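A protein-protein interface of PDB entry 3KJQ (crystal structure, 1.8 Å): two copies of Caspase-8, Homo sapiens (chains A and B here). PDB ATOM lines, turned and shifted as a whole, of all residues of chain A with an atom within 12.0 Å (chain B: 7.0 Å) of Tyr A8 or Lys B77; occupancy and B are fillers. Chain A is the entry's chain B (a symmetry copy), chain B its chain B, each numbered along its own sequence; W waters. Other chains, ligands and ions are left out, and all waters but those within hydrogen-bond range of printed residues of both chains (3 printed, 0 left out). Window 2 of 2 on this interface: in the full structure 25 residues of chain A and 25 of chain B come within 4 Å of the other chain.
The side-chain amino group (NZ) of Lys B77 lies within hydrogen-bond range of the backbone carbonyl oxygen (O) of Tyr A8 (2.8 Å).
O of Thr A85 sits at hydrogen-bond distance from N of Asp A14 (3.0 Å).
The backbone carbonyl oxygen (O) of Lys B69 lies within hydrogen-bond range of the side-chain amino group (NZ) of Lys B77 (2.9 Å).
The side-chain sulfur of Met B79 sits close to the side-chain hydroxyl of Ser B67 (3.5 Å).
The backbone carbonyl oxygen of Ser B67 is in hydrogen-bond range of the side-chain amino group of Lys B77.
The backbone NH (N) of Tyr B28 sits at hydrogen-bond distance from the side-chain amide oxygen (OE1) of Gln B78, 2.9 Å away.
The side-chain carboxylate (OD1) of Asp A14 lies within salt-bridge range of the guanidinium group (NE) of Arg A87 (2.8 Å).
O of Ser B67 touches O of Tyr A8, 3.5 Å away.
O of Ser B67 touches CA of Ile A9, 3.8 Å away.
Ile A9 touches Lys B77 (CA to CE, 3.8 Å).
CD of Pro A10 touches OG of Ser B67, at 3.3 Å.
Pro A10 touches Gln B78 (CG to O, 3.5 Å).
Pro A10 touches Met B79 (CB to CB, 3.7 Å).
Glu A12 touches Met B79 (O to CG, 3.9 Å).
Ala A13 touches Met B79.
Thr A85 touches Met B79 (O to CE, 3.6 Å).
Arg A87 touches Ser B67 (CD to OG, 3.2 Å).
Of chain B, only Ser B67 (3.5 Å) and Lys B77 (2.8 Å) come within 4 Å of Tyr A8.
Printed residues of chain B within 4 Å of Ile A9: Ser B67 (3.8 Å) and Lys B77 (3.8 Å).
Of the printed residues of chain B, Ala A13 touches Met B79.
No residue of chain A comes within 4 Å of Val B26.
No residue of chain A comes within 4 Å of Asn B68.
Asp B70 touches none of the printed residues of chain A.
No residue of chain A comes within 4 Å of Asp B71.
Of chain A, only Tyr A8 (2.8 Å) and Ile A9 (3.8 Å) come within 4 Å of Lys B77.
Printed residues of chain A within 4 Å of Met B79: Pro A10 (3.7 Å), Glu A12 (3.9 Å), Ala A13 (3.5 Å) and Thr A85 (3.6 Å).
The nearest residue of chain B that does not touch Tyr A8 is Asn B68 (4.6 Å).
The nearest residue of chain A that does not touch Lys B77 is Pro A10 (4.03 Å).
Of the 18 printed residues of chain B, 4 touch a printed residue of chain A.
Printed residues of chain B that touch a printed residue of chain A: Ser B67, Lys B77, Gln B78 and Met B79.
Hydrophobic or aromatic side chains of chain B within 4 Å of the printed part of chain A: Met B79.
Of the 12 printed residues of chain A, 7 touch a printed residue of chain B.
Hydrophobic or aromatic side chains of chain A within 4 Å of the printed part of chain B: Pro A10 and Ala A13.
Among the printed residues, 11 pairs touch across the chains.
No position is printed for both chains.
Of the 11 pairs that touch across the chains among the printed residues, none has its exchanged pair printed and touching as well.
Water W1 bridges OD1 of Asn B68 (2.7 Å) and NH1 of Arg A87 (2.9 Å).
Water W3 bridges OE2 of Glu A12 and SG of Cys B25.
Water W2 lies within hydrogen-bond range of the backbone carbonyl oxygen (O) of Tyr A8 (2.8 Å) and the side-chain amide oxygen (OD1) of Asn B68 (2.8 Å).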
ATOM      1  N   THR A   6      -8.656  11.531   6.551  1.00  0.00           N
ATOM      2  CA  THR A   6      -8.310  12.327   7.725  1.00  0.00           C
ATOM      3  C   THR A   6      -8.292  11.436   8.968  1.00  0.00           C
ATOM      4  O   THR A   6      -8.615  10.242   8.896  1.00  0.00           O
ATOM      5  CB  THR A   6      -9.280  13.536   7.911  1.00  0.00           C
ATOM      6  OG1 THR A   6     -10.481  13.135   8.594  1.00  0.00           O
ATOM      7  CG2 THR A   6      -9.634  14.150   6.558  1.00  0.00           C
ATOM      8  N   ARG A   7      -7.917  12.019  10.103  1.00  0.00           N
ATOM      9  CA  ARG A   7      -7.856  11.284  11.357  1.00  0.00           C
ATOM     10  C   ARG A   7      -9.043  11.674  12.220  1.00  0.00           C
ATOM     11  O   ARG A   7      -9.568  12.782  12.095  1.00  0.00           O
ATOM     12  CB  ARG A   7      -6.560  11.603  12.099  1.00  0.00           C
ATOM     13  CG  ARG A   7      -5.302  11.235  11.336  1.00  0.00           C
ATOM     14  CD  ARG A   7      -5.012   9.737  11.372  1.00  0.00           C
ATOM     15  NE  ARG A   7      -3.959   9.375  10.419  1.00  0.00           N
ATOM     16  CZ  ARG A   7      -2.648   9.503  10.629  1.00  0.00           C
ATOM     17  NH1 ARG A   7      -1.792   9.145   9.673  1.00  0.00           N
ATOM     18  NH2 ARG A   7      -2.175   9.984  11.778  1.00  0.00           N
ATOM     19  N   TYR A   8      -9.438  10.769  13.108  1.00  0.00           N
ATOM     20  CA  TYR A   8     -10.511  11.017  14.051  1.00  0.00           C
ATOM     21  C   TYR A   8     -10.014  10.889  15.491  1.00  0.00           C
ATOM     22  O   TYR A   8      -9.269   9.969  15.823  1.00  0.00           O
ATOM     23  CB  TYR A   8     -11.674  10.056  13.787  1.00  0.00           C
ATOM     24  CG  TYR A   8     -12.295  10.342  12.444  1.00  0.00           C
ATOM     25  CD1 TYR A   8     -11.721   9.854  11.273  1.00  0.00           C
ATOM     26  CD2 TYR A   8     -13.398  11.179  12.333  1.00  0.00           C
ATOM     27  CE1 TYR A   8     -12.266  10.147  10.025  1.00  0.00           C
ATOM     28  CE2 TYR A   8     -13.948  11.484  11.097  1.00  0.00           C
ATOM     29  CZ  TYR A   8     -13.380  10.967   9.947  1.00  0.00           C
ATOM     30  OH  TYR A   8     -13.930  11.276   8.716  1.00  0.00           O
ATOM     31  N   ILE A   9     -10.438  11.826  16.331  1.00  0.00           N
ATOM     32  CA  ILE A   9     -10.168  11.773  17.767  1.00  0.00           C
ATOM     33  C   ILE A   9     -11.519  11.838  18.493  1.00  0.00           C
ATOM     34  O   ILE A   9     -12.535  12.119  17.868  1.00  0.00           O
ATOM     35  CB  ILE A   9      -9.222  12.921  18.203  1.00  0.00           C
ATOM     36  CG1 ILE A   9      -9.866  14.298  17.964  1.00  0.00           C
ATOM     37  CG2 ILE A   9      -7.891  12.791  17.478  1.00  0.00           C
ATOM     38  CD1 ILE A   9      -9.024  15.514  18.483  1.00  0.00           C
ATOM     39  N   PRO A  10     -11.541  11.528  19.800  1.00  0.00           N
ATOM     40  CA  PRO A  10     -12.798  11.583  20.523  1.00  0.00           C
ATOM     41  C   PRO A  10     -13.451  12.966  20.582  1.00  0.00           C
ATOM     42  O   PRO A  10     -12.760  14.005  20.660  1.00  0.00           O
ATOM     43  CB  PRO A  10     -12.401  11.123  21.934  1.00  0.00           C
ATOM     44  CG  PRO A  10     -11.197  10.329  21.733  1.00  0.00           C
ATOM     45  CD  PRO A  10     -10.457  11.037  20.668  1.00  0.00           C
ATOM     46  N   ASP A  11     -14.781  12.945  20.567  1.00  0.00           N
ATOM     47  CA  ASP A  11     -15.623  14.151  20.687  1.00  0.00           C
ATOM     48  C   ASP A  11     -15.239  15.020  21.906  1.00  0.00           C
ATOM     49  O   ASP A  11     -15.276  16.248  21.834  1.00  0.00           O
ATOM     50  CB  ASP A  11     -17.084  13.701  20.792  1.00  0.00           C
ATOM     51  CG  ASP A  11     -18.074  14.847  20.745  1.00  0.00           C
ATOM     52  OD1 ASP A  11     -17.807  15.851  20.055  1.00  0.00           O
ATOM     53  OD2 ASP A  11     -19.134  14.714  21.391  1.00  0.00           O
ATOM     54  N   GLU A  12     -14.870  14.370  23.009  1.00  0.00           N
ATOM     55  CA  GLU A  12     -14.565  15.049  24.282  1.00  0.00           C
ATOM     56  C   GLU A  12     -13.062  15.207  24.553  1.00  0.00           C
ATOM     57  O   GLU A  12     -12.648  15.402  25.706  1.00  0.00           O
ATOM     58  CB  GLU A  12     -15.232  14.298  25.435  1.00  0.00           C
ATOM     59  CG  GLU A  12     -16.753  14.382  25.396  1.00  0.00           C
ATOM     60  CD  GLU A  12     -17.433  13.567  26.478  1.00  0.00           C
ATOM     61  OE1 GLU A  12     -17.113  13.754  27.675  1.00  0.00           O
ATOM     62  OE2 GLU A  12     -18.323  12.751  26.132  1.00  0.00           O
ATOM     63  N   ALA A  13     -12.249  15.134  23.502  1.00  0.00           N
ATOM     64  CA  ALA A  13     -10.810  15.336  23.643  1.00  0.00           C
ATOM     65  C   ALA A  13     -10.455  16.805  23.896  1.00  0.00           C
ATOM     66  O   ALA A  13     -11.251  17.705  23.613  1.00  0.00           O
ATOM     67  CB  ALA A  13     -10.068  14.842  22.422  1.00  0.00           C
ATOM     68  N   ASP A  14      -9.252  17.024  24.426  1.00  0.00           N
ATOM     69  CA  ASP A  14      -8.624  18.337  24.499  1.00  0.00           C
ATOM     70  C   ASP A  14      -9.286  19.333  25.458  1.00  0.00           C
ATOM     71  O   ASP A  14      -9.194  20.546  25.235  1.00  0.00           O
ATOM     72  CB  ASP A  14      -8.503  18.962  23.098  1.00  0.00           C
ATOM     73  CG  ASP A  14      -7.885  18.008  22.082  1.00  0.00           C
ATOM     74  OD1 ASP A  14      -6.804  17.434  22.354  1.00  0.00           O
ATOM     75  OD2 ASP A  14      -8.491  17.811  21.011  1.00  0.00           O
ATOM     76  N   THR A  85      -8.713  15.906  29.510  1.00  0.00           N
ATOM     77  CA  THR A  85      -8.657  15.005  28.363  1.00  0.00           C
ATOM     78  C   THR A  85      -7.640  15.519  27.329  1.00  0.00           C
ATOM     79  O   THR A  85      -7.662  15.113  26.170  1.00  0.00           O
ATOM     80  CB  THR A  85     -10.049  14.807  27.713  1.00  0.00           C
ATOM     81  OG1 THR A  85     -10.582  16.077  27.277  1.00  0.00           O
ATOM     82  CG2 THR A  85     -11.008  14.135  28.684  1.00  0.00           C
ATOM     83  N   ARG A  87      -4.434  15.888  25.103  1.00  0.00           N
ATOM     84  CA  ARG A  87      -3.642  14.876  24.404  1.00  0.00           C
ATOM     85  C   ARG A  87      -2.216  15.339  24.109  1.00  0.00           C
ATOM     86  O   ARG A  87      -1.389  14.555  23.609  1.00  0.00           O
ATOM     87  CB  ARG A  87      -4.323  14.508  23.083  1.00  0.00           C
ATOM     88  CG  ARG A  87      -5.679  13.829  23.189  1.00  0.00           C
ATOM     89  CD  ARG A  87      -6.342  13.677  21.823  1.00  0.00           C
ATOM     90  NE  ARG A  87      -6.418  14.956  21.131  1.00  0.00           N
ATOM     91  CZ  ARG A  87      -5.698  15.307  20.064  1.00  0.00           C
ATOM     92  NH1 ARG A  87      -4.857  14.471  19.453  1.00  0.00           N
ATOM     93  NH2 ARG A  87      -5.841  16.514  19.571  1.00  0.00           N
ATOM     94  N   LYS A  88      -1.935  16.606  24.394  1.00  0.00           N
ATOM     95  CA  LYS A  88      -0.625  17.206  24.195  1.00  0.00           C
ATOM     96  C   LYS A  88      -0.336  18.127  25.376  1.00  0.00           C
ATOM     97  O   LYS A  88      -1.235  18.448  26.167  1.00  0.00           O
ATOM     98  CB  LYS A  88      -0.579  18.023  22.897  1.00  0.00           C
ATOM     99  CG  LYS A  88      -1.060  17.293  21.641  1.00  0.00           C
ATOM    100  CD  LYS A  88      -1.125  18.206  20.408  1.00  0.00           C
ATOM    101  CE  LYS A  88      -1.529  17.430  19.155  1.00  0.00           C
ATOM    102  NZ  LYS A  88      -1.488  18.299  17.931  1.00  0.00           N
ATOM    103  N   THR B  21     -11.894   6.048  30.793  1.00  0.00           N
ATOM    104  CA  THR B  21     -12.870   6.756  29.960  1.00  0.00           C
ATOM    105  C   THR B  21     -13.543   7.896  30.719  1.00  0.00           C
ATOM    106  O   THR B  21     -13.716   7.831  31.935  1.00  0.00           O
ATOM    107  CB  THR B  21     -13.988   5.804  29.443  1.00  0.00           C
ATOM    108  OG1 THR B  21     -15.012   6.556  28.768  1.00  0.00           O
ATOM    109  CG2 THR B  21     -14.606   5.047  30.580  1.00  0.00           C
ATOM    110  N   CYS B  25     -19.513   6.686  29.112  1.00  0.00           N
ATOM    111  CA  CYS B  25     -19.060   5.996  27.906  1.00  0.00           C
ATOM    112  C   CYS B  25     -18.300   4.709  28.186  1.00  0.00           C
ATOM    113  O   CYS B  25     -17.868   4.458  29.305  1.00  0.00           O
ATOM    114  CB  CYS B  25     -18.192   6.920  27.050  1.00  0.00           C
ATOM    115  SG  CYS B  25     -19.084   8.376  26.480  1.00  0.00           S
ATOM    116  N   VAL B  26     -18.145   3.920  27.130  1.00  0.00           N
ATOM    117  CA  VAL B  26     -17.480   2.624  27.203  1.00  0.00           C
ATOM    118  C   VAL B  26     -15.952   2.758  27.136  1.00  0.00           C
ATOM    119  O   VAL B  26     -15.414   3.760  26.656  1.00  0.00           O
ATOM    120  CB  VAL B  26     -17.982   1.655  26.074  1.00  0.00           C
ATOM    121  CG1 VAL B  26     -19.505   1.464  26.156  1.00  0.00           C
ATOM    122  CG2 VAL B  26     -17.557   2.145  24.684  1.00  0.00           C
ATOM    123  N   SER B  27     -15.261   1.752  27.661  1.00  0.00           N
ATOM    124  CA  SER B  27     -13.862   1.523  27.352  1.00  0.00           C
ATOM    125  C   SER B  27     -13.747   0.115  26.750  1.00  0.00           C
ATOM    126  O   SER B  27     -14.668  -0.704  26.883  1.00  0.00           O
ATOM    127  CB  SER B  27     -12.984   1.674  28.603  1.00  0.00           C
ATOM    128  OG  SER B  27     -13.254   0.657  29.550  1.00  0.00           O
ATOM    129  N   TYR B  28     -12.618  -0.150  26.100  1.00  0.00           N
ATOM    130  CA  TYR B  28     -12.461  -1.319  25.247  1.00  0.00           C
ATOM    131  C   TYR B  28     -11.380  -2.270  25.720  1.00  0.00           C
ATOM    132  O   TYR B  28     -10.319  -1.844  26.205  1.00  0.00           O
ATOM    133  CB  TYR B  28     -12.135  -0.871  23.822  1.00  0.00           C
ATOM    134  CG  TYR B  28     -13.296  -0.198  23.152  1.00  0.00           C
ATOM    135  CD1 TYR B  28     -14.293  -0.945  22.547  1.00  0.00           C
ATOM    136  CD2 TYR B  28     -13.409   1.189  23.132  1.00  0.00           C
ATOM    137  CE1 TYR B  28     -15.380  -0.334  21.925  1.00  0.00           C
ATOM    138  CE2 TYR B  28     -14.492   1.813  22.520  1.00  0.00           C
ATOM    139  CZ  TYR B  28     -15.481   1.039  21.916  1.00  0.00           C
ATOM    140  OH  TYR B  28     -16.566   1.648  21.285  1.00  0.00           O
ATOM    141  N   TRP B  36      -7.221  -1.166  25.853  1.00  0.00           N
ATOM    142  CA  TRP B  36      -6.579  -0.016  25.233  1.00  0.00           C
ATOM    143  C   TRP B  36      -5.838   0.813  26.274  1.00  0.00           C
ATOM    144  O   TRP B  36      -4.683   1.177  26.080  1.00  0.00           O
ATOM    145  CB  TRP B  36      -7.621   0.854  24.537  1.00  0.00           C
ATOM    146  CG  TRP B  36      -8.232   0.260  23.317  1.00  0.00           C
ATOM    147  CD1 TRP B  36      -8.045  -0.990  22.800  1.00  0.00           C
ATOM    148  CD2 TRP B  36      -9.165   0.918  22.460  1.00  0.00           C
ATOM    149  NE1 TRP B  36      -8.807  -1.142  21.649  1.00  0.00           N
ATOM    150  CE2 TRP B  36      -9.507   0.018  21.433  1.00  0.00           C
ATOM    151  CE3 TRP B  36      -9.750   2.187  22.472  1.00  0.00           C
ATOM    152  CZ2 TRP B  36     -10.402   0.358  20.414  1.00  0.00           C
ATOM    153  CZ3 TRP B  36     -10.629   2.522  21.468  1.00  0.00           C
ATOM    154  CH2 TRP B  36     -10.948   1.611  20.449  1.00  0.00           C
ATOM    155  N   VAL B  66      -4.588   6.470  23.070  1.00  0.00           N
ATOM    156  CA  VAL B  66      -5.910   5.864  23.120  1.00  0.00           C
ATOM    157  C   VAL B  66      -6.878   6.650  22.206  1.00  0.00           C
ATOM    158  O   VAL B  66      -7.728   6.045  21.545  1.00  0.00           O
ATOM    159  CB  VAL B  66      -6.431   5.729  24.575  1.00  0.00           C
ATOM    160  CG1 VAL B  66      -7.865   5.216  24.613  1.00  0.00           C
ATOM    161  CG2 VAL B  66      -5.513   4.798  25.389  1.00  0.00           C
ATOM    162  N   SER B  67      -6.707   7.973  22.127  1.00  0.00           N
ATOM    163  CA  SER B  67      -7.540   8.818  21.238  1.00  0.00           C
ATOM    164  C   SER B  67      -7.424   8.439  19.760  1.00  0.00           C
ATOM    165  O   SER B  67      -8.335   8.720  18.989  1.00  0.00           O
ATOM    166  CB  SER B  67      -7.193  10.304  21.382  1.00  0.00           C
ATOM    167  OG  SER B  67      -7.747  10.845  22.571  1.00  0.00           O
ATOM    168  N   ASN B  68      -6.305   7.826  19.377  1.00  0.00           N
ATOM    169  CA  ASN B  68      -6.075   7.410  17.986  1.00  0.00           C
ATOM    170  C   ASN B  68      -6.556   6.017  17.629  1.00  0.00           C
ATOM    171  O   ASN B  68      -6.451   5.608  16.466  1.00  0.00           O
ATOM    172  CB  ASN B  68      -4.598   7.522  17.653  1.00  0.00           C
ATOM    173  CG  ASN B  68      -4.130   8.958  17.560  1.00  0.00           C
ATOM    174  OD1 ASN B  68      -4.925   9.885  17.369  1.00  0.00           O
ATOM    175  ND2 ASN B  68      -2.823   9.148  17.688  1.00  0.00           N
ATOM    176  N   LYS B  69      -7.066   5.282  18.611  1.00  0.00           N
ATOM    177  CA  LYS B  69      -7.624   3.960  18.385  1.00  0.00           C
ATOM    178  C   LYS B  69      -9.105   4.044  18.017  1.00  0.00           C
ATOM    179  O   LYS B  69      -9.793   5.025  18.331  1.00  0.00           O
ATOM    180  CB  LYS B  69      -7.455   3.094  19.634  1.00  0.00           C
ATOM    181  CG  LYS B  69      -6.011   2.834  19.989  1.00  0.00           C
ATOM    182  CD  LYS B  69      -5.877   1.767  21.071  1.00  0.00           C
ATOM    183  CE  LYS B  69      -4.677   0.842  20.803  1.00  0.00           C
ATOM    184  NZ  LYS B  69      -4.865  -0.091  19.631  1.00  0.00           N
ATOM    185  N   ASP B  70      -9.615   3.007  17.364  1.00  0.00           N
ATOM    186  CA  ASP B  70     -11.044   2.981  17.077  1.00  0.00           C
ATOM    187  C   ASP B  70     -11.658   1.600  17.073  1.00  0.00           C
ATOM    188  O   ASP B  70     -10.992   0.590  16.846  1.00  0.00           O
ATOM    189  CB  ASP B  70     -11.343   3.691  15.766  1.00  0.00           C
ATOM    190  CG  ASP B  70     -10.323   3.392  14.721  1.00  0.00           C
ATOM    191  OD1 ASP B  70     -10.186   2.195  14.401  1.00  0.00           O
ATOM    192  OD2 ASP B  70      -9.643   4.340  14.253  1.00  0.00           O
ATOM    193  N   ASP B  71     -12.947   1.613  17.361  1.00  0.00           N
ATOM    194  CA  ASP B  71     -13.814   0.458  17.331  1.00  0.00           C
ATOM    195  C   ASP B  71     -14.530   0.552  15.978  1.00  0.00           C
ATOM    196  O   ASP B  71     -15.483   1.318  15.823  1.00  0.00           O
ATOM    197  CB  ASP B  71     -14.773   0.547  18.523  1.00  0.00           C
ATOM    198  CG  ASP B  71     -16.059  -0.230  18.327  1.00  0.00           C
ATOM    199  OD1 ASP B  71     -16.136  -1.054  17.391  1.00  0.00           O
ATOM    200  OD2 ASP B  71     -16.996  -0.007  19.128  1.00  0.00           O
ATOM    201  N   ASN B  74     -18.491  -0.006  15.464  1.00  0.00           N
ATOM    202  CA  ASN B  74     -19.436   1.046  15.838  1.00  0.00           C
ATOM    203  C   ASN B  74     -18.941   2.455  15.502  1.00  0.00           C
ATOM    204  O   ASN B  74     -19.620   3.422  15.828  1.00  0.00           O
ATOM    205  CB  ASN B  74     -19.705   0.975  17.346  1.00  0.00           C
ATOM    206  CG  ASN B  74     -20.290  -0.363  17.787  1.00  0.00           C
ATOM    207  OD1 ASN B  74     -19.664  -1.107  18.549  1.00  0.00           O
ATOM    208  ND2 ASN B  74     -21.493  -0.672  17.313  1.00  0.00           N
ATOM    209  N   MET B  75     -17.780   2.565  14.860  1.00  0.00           N
ATOM    210  CA  MET B  75     -17.065   3.844  14.719  1.00  0.00           C
ATOM    211  C   MET B  75     -16.956   4.519  16.089  1.00  0.00           C
ATOM    212  O   MET B  75     -17.260   5.712  16.244  1.00  0.00           O
ATOM    213  CB  MET B  75     -17.756   4.771  13.713  1.00  0.00           C
ATOM    214  CG  MET B  75     -18.000   4.144  12.345  1.00  0.00           C
ATOM    215  SD  MET B  75     -16.500   3.587  11.528  1.00  0.00           S
ATOM    216  CE  MET B  75     -17.202   2.830  10.071  1.00  0.00           C
ATOM    217  N   GLY B  76     -16.538   3.727  17.077  1.00  0.00           N
ATOM    218  CA  GLY B  76     -16.449   4.175  18.461  1.00  0.00           C
ATOM    219  C   GLY B  76     -15.038   4.602  18.808  1.00  0.00           C
ATOM    220  O   GLY B  76     -14.063   4.116  18.226  1.00  0.00           O
ATOM    221  N   LYS B  77     -14.941   5.529  19.754  1.00  0.00           N
ATOM    222  CA  LYS B  77     -13.657   6.028  20.227  1.00  0.00           C
ATOM    223  C   LYS B  77     -13.621   5.857  21.736  1.00  0.00           C
ATOM    224  O   LYS B  77     -14.611   5.465  22.343  1.00  0.00           O
ATOM    225  CB  LYS B  77     -13.478   7.509  19.873  1.00  0.00           C
ATOM    226  CG  LYS B  77     -13.554   7.837  18.383  1.00  0.00           C
ATOM    227  CD  LYS B  77     -12.376   7.247  17.610  1.00  0.00           C
ATOM    228  CE  LYS B  77     -11.154   8.127  17.667  1.00  0.00           C
ATOM    229  NZ  LYS B  77      -9.971   7.563  16.959  1.00  0.00           N
ATOM    230  N   GLN B  78     -12.475   6.162  22.333  1.00  0.00           N
ATOM    231  CA  GLN B  78     -12.341   6.110  23.779  1.00  0.00           C
ATOM    232  C   GLN B  78     -11.463   7.267  24.233  1.00  0.00           C
ATOM    233  O   GLN B  78     -10.386   7.485  23.674  1.00  0.00           O
ATOM    234  CB  GLN B  78     -11.708   4.785  24.210  1.00  0.00           C
ATOM    235  CG  GLN B  78     -11.621   4.605  25.716  1.00  0.00           C
ATOM    236  CD  GLN B  78     -10.985   3.288  26.118  1.00  0.00           C
ATOM    237  OE1 GLN B  78     -11.199   2.261  25.474  1.00  0.00           O
ATOM    238  NE2 GLN B  78     -10.194   3.313  27.188  1.00  0.00           N
ATOM    239  N   MET B  79     -11.924   7.981  25.261  1.00  0.00           N
ATOM    240  CA  MET B  79     -11.229   9.157  25.786  1.00  0.00           C
ATOM    241  C   MET B  79     -10.928   8.977  27.279  1.00  0.00           C
ATOM    242  O   MET B  79     -11.815   9.146  28.119  1.00  0.00           O
ATOM    243  CB  MET B  79     -12.093  10.410  25.600  1.00  0.00           C
ATOM    244  CG  MET B  79     -11.414  11.730  25.965  1.00  0.00           C
ATOM    245  SD  MET B  79     -10.069  12.146  24.835  1.00  0.00           S
ATOM    246  CE  MET B  79      -8.590  11.710  25.766  1.00  0.00           C
HETATM  247  O   HOH W   1      -4.708  11.529  19.459  1.00  0.00           O
HETATM  248  O   HOH W   2      -6.571   9.712  15.072  1.00  0.00           O
HETATM  249  O   HOH W   3     -20.204  11.466  27.654  1.00  0.00           O
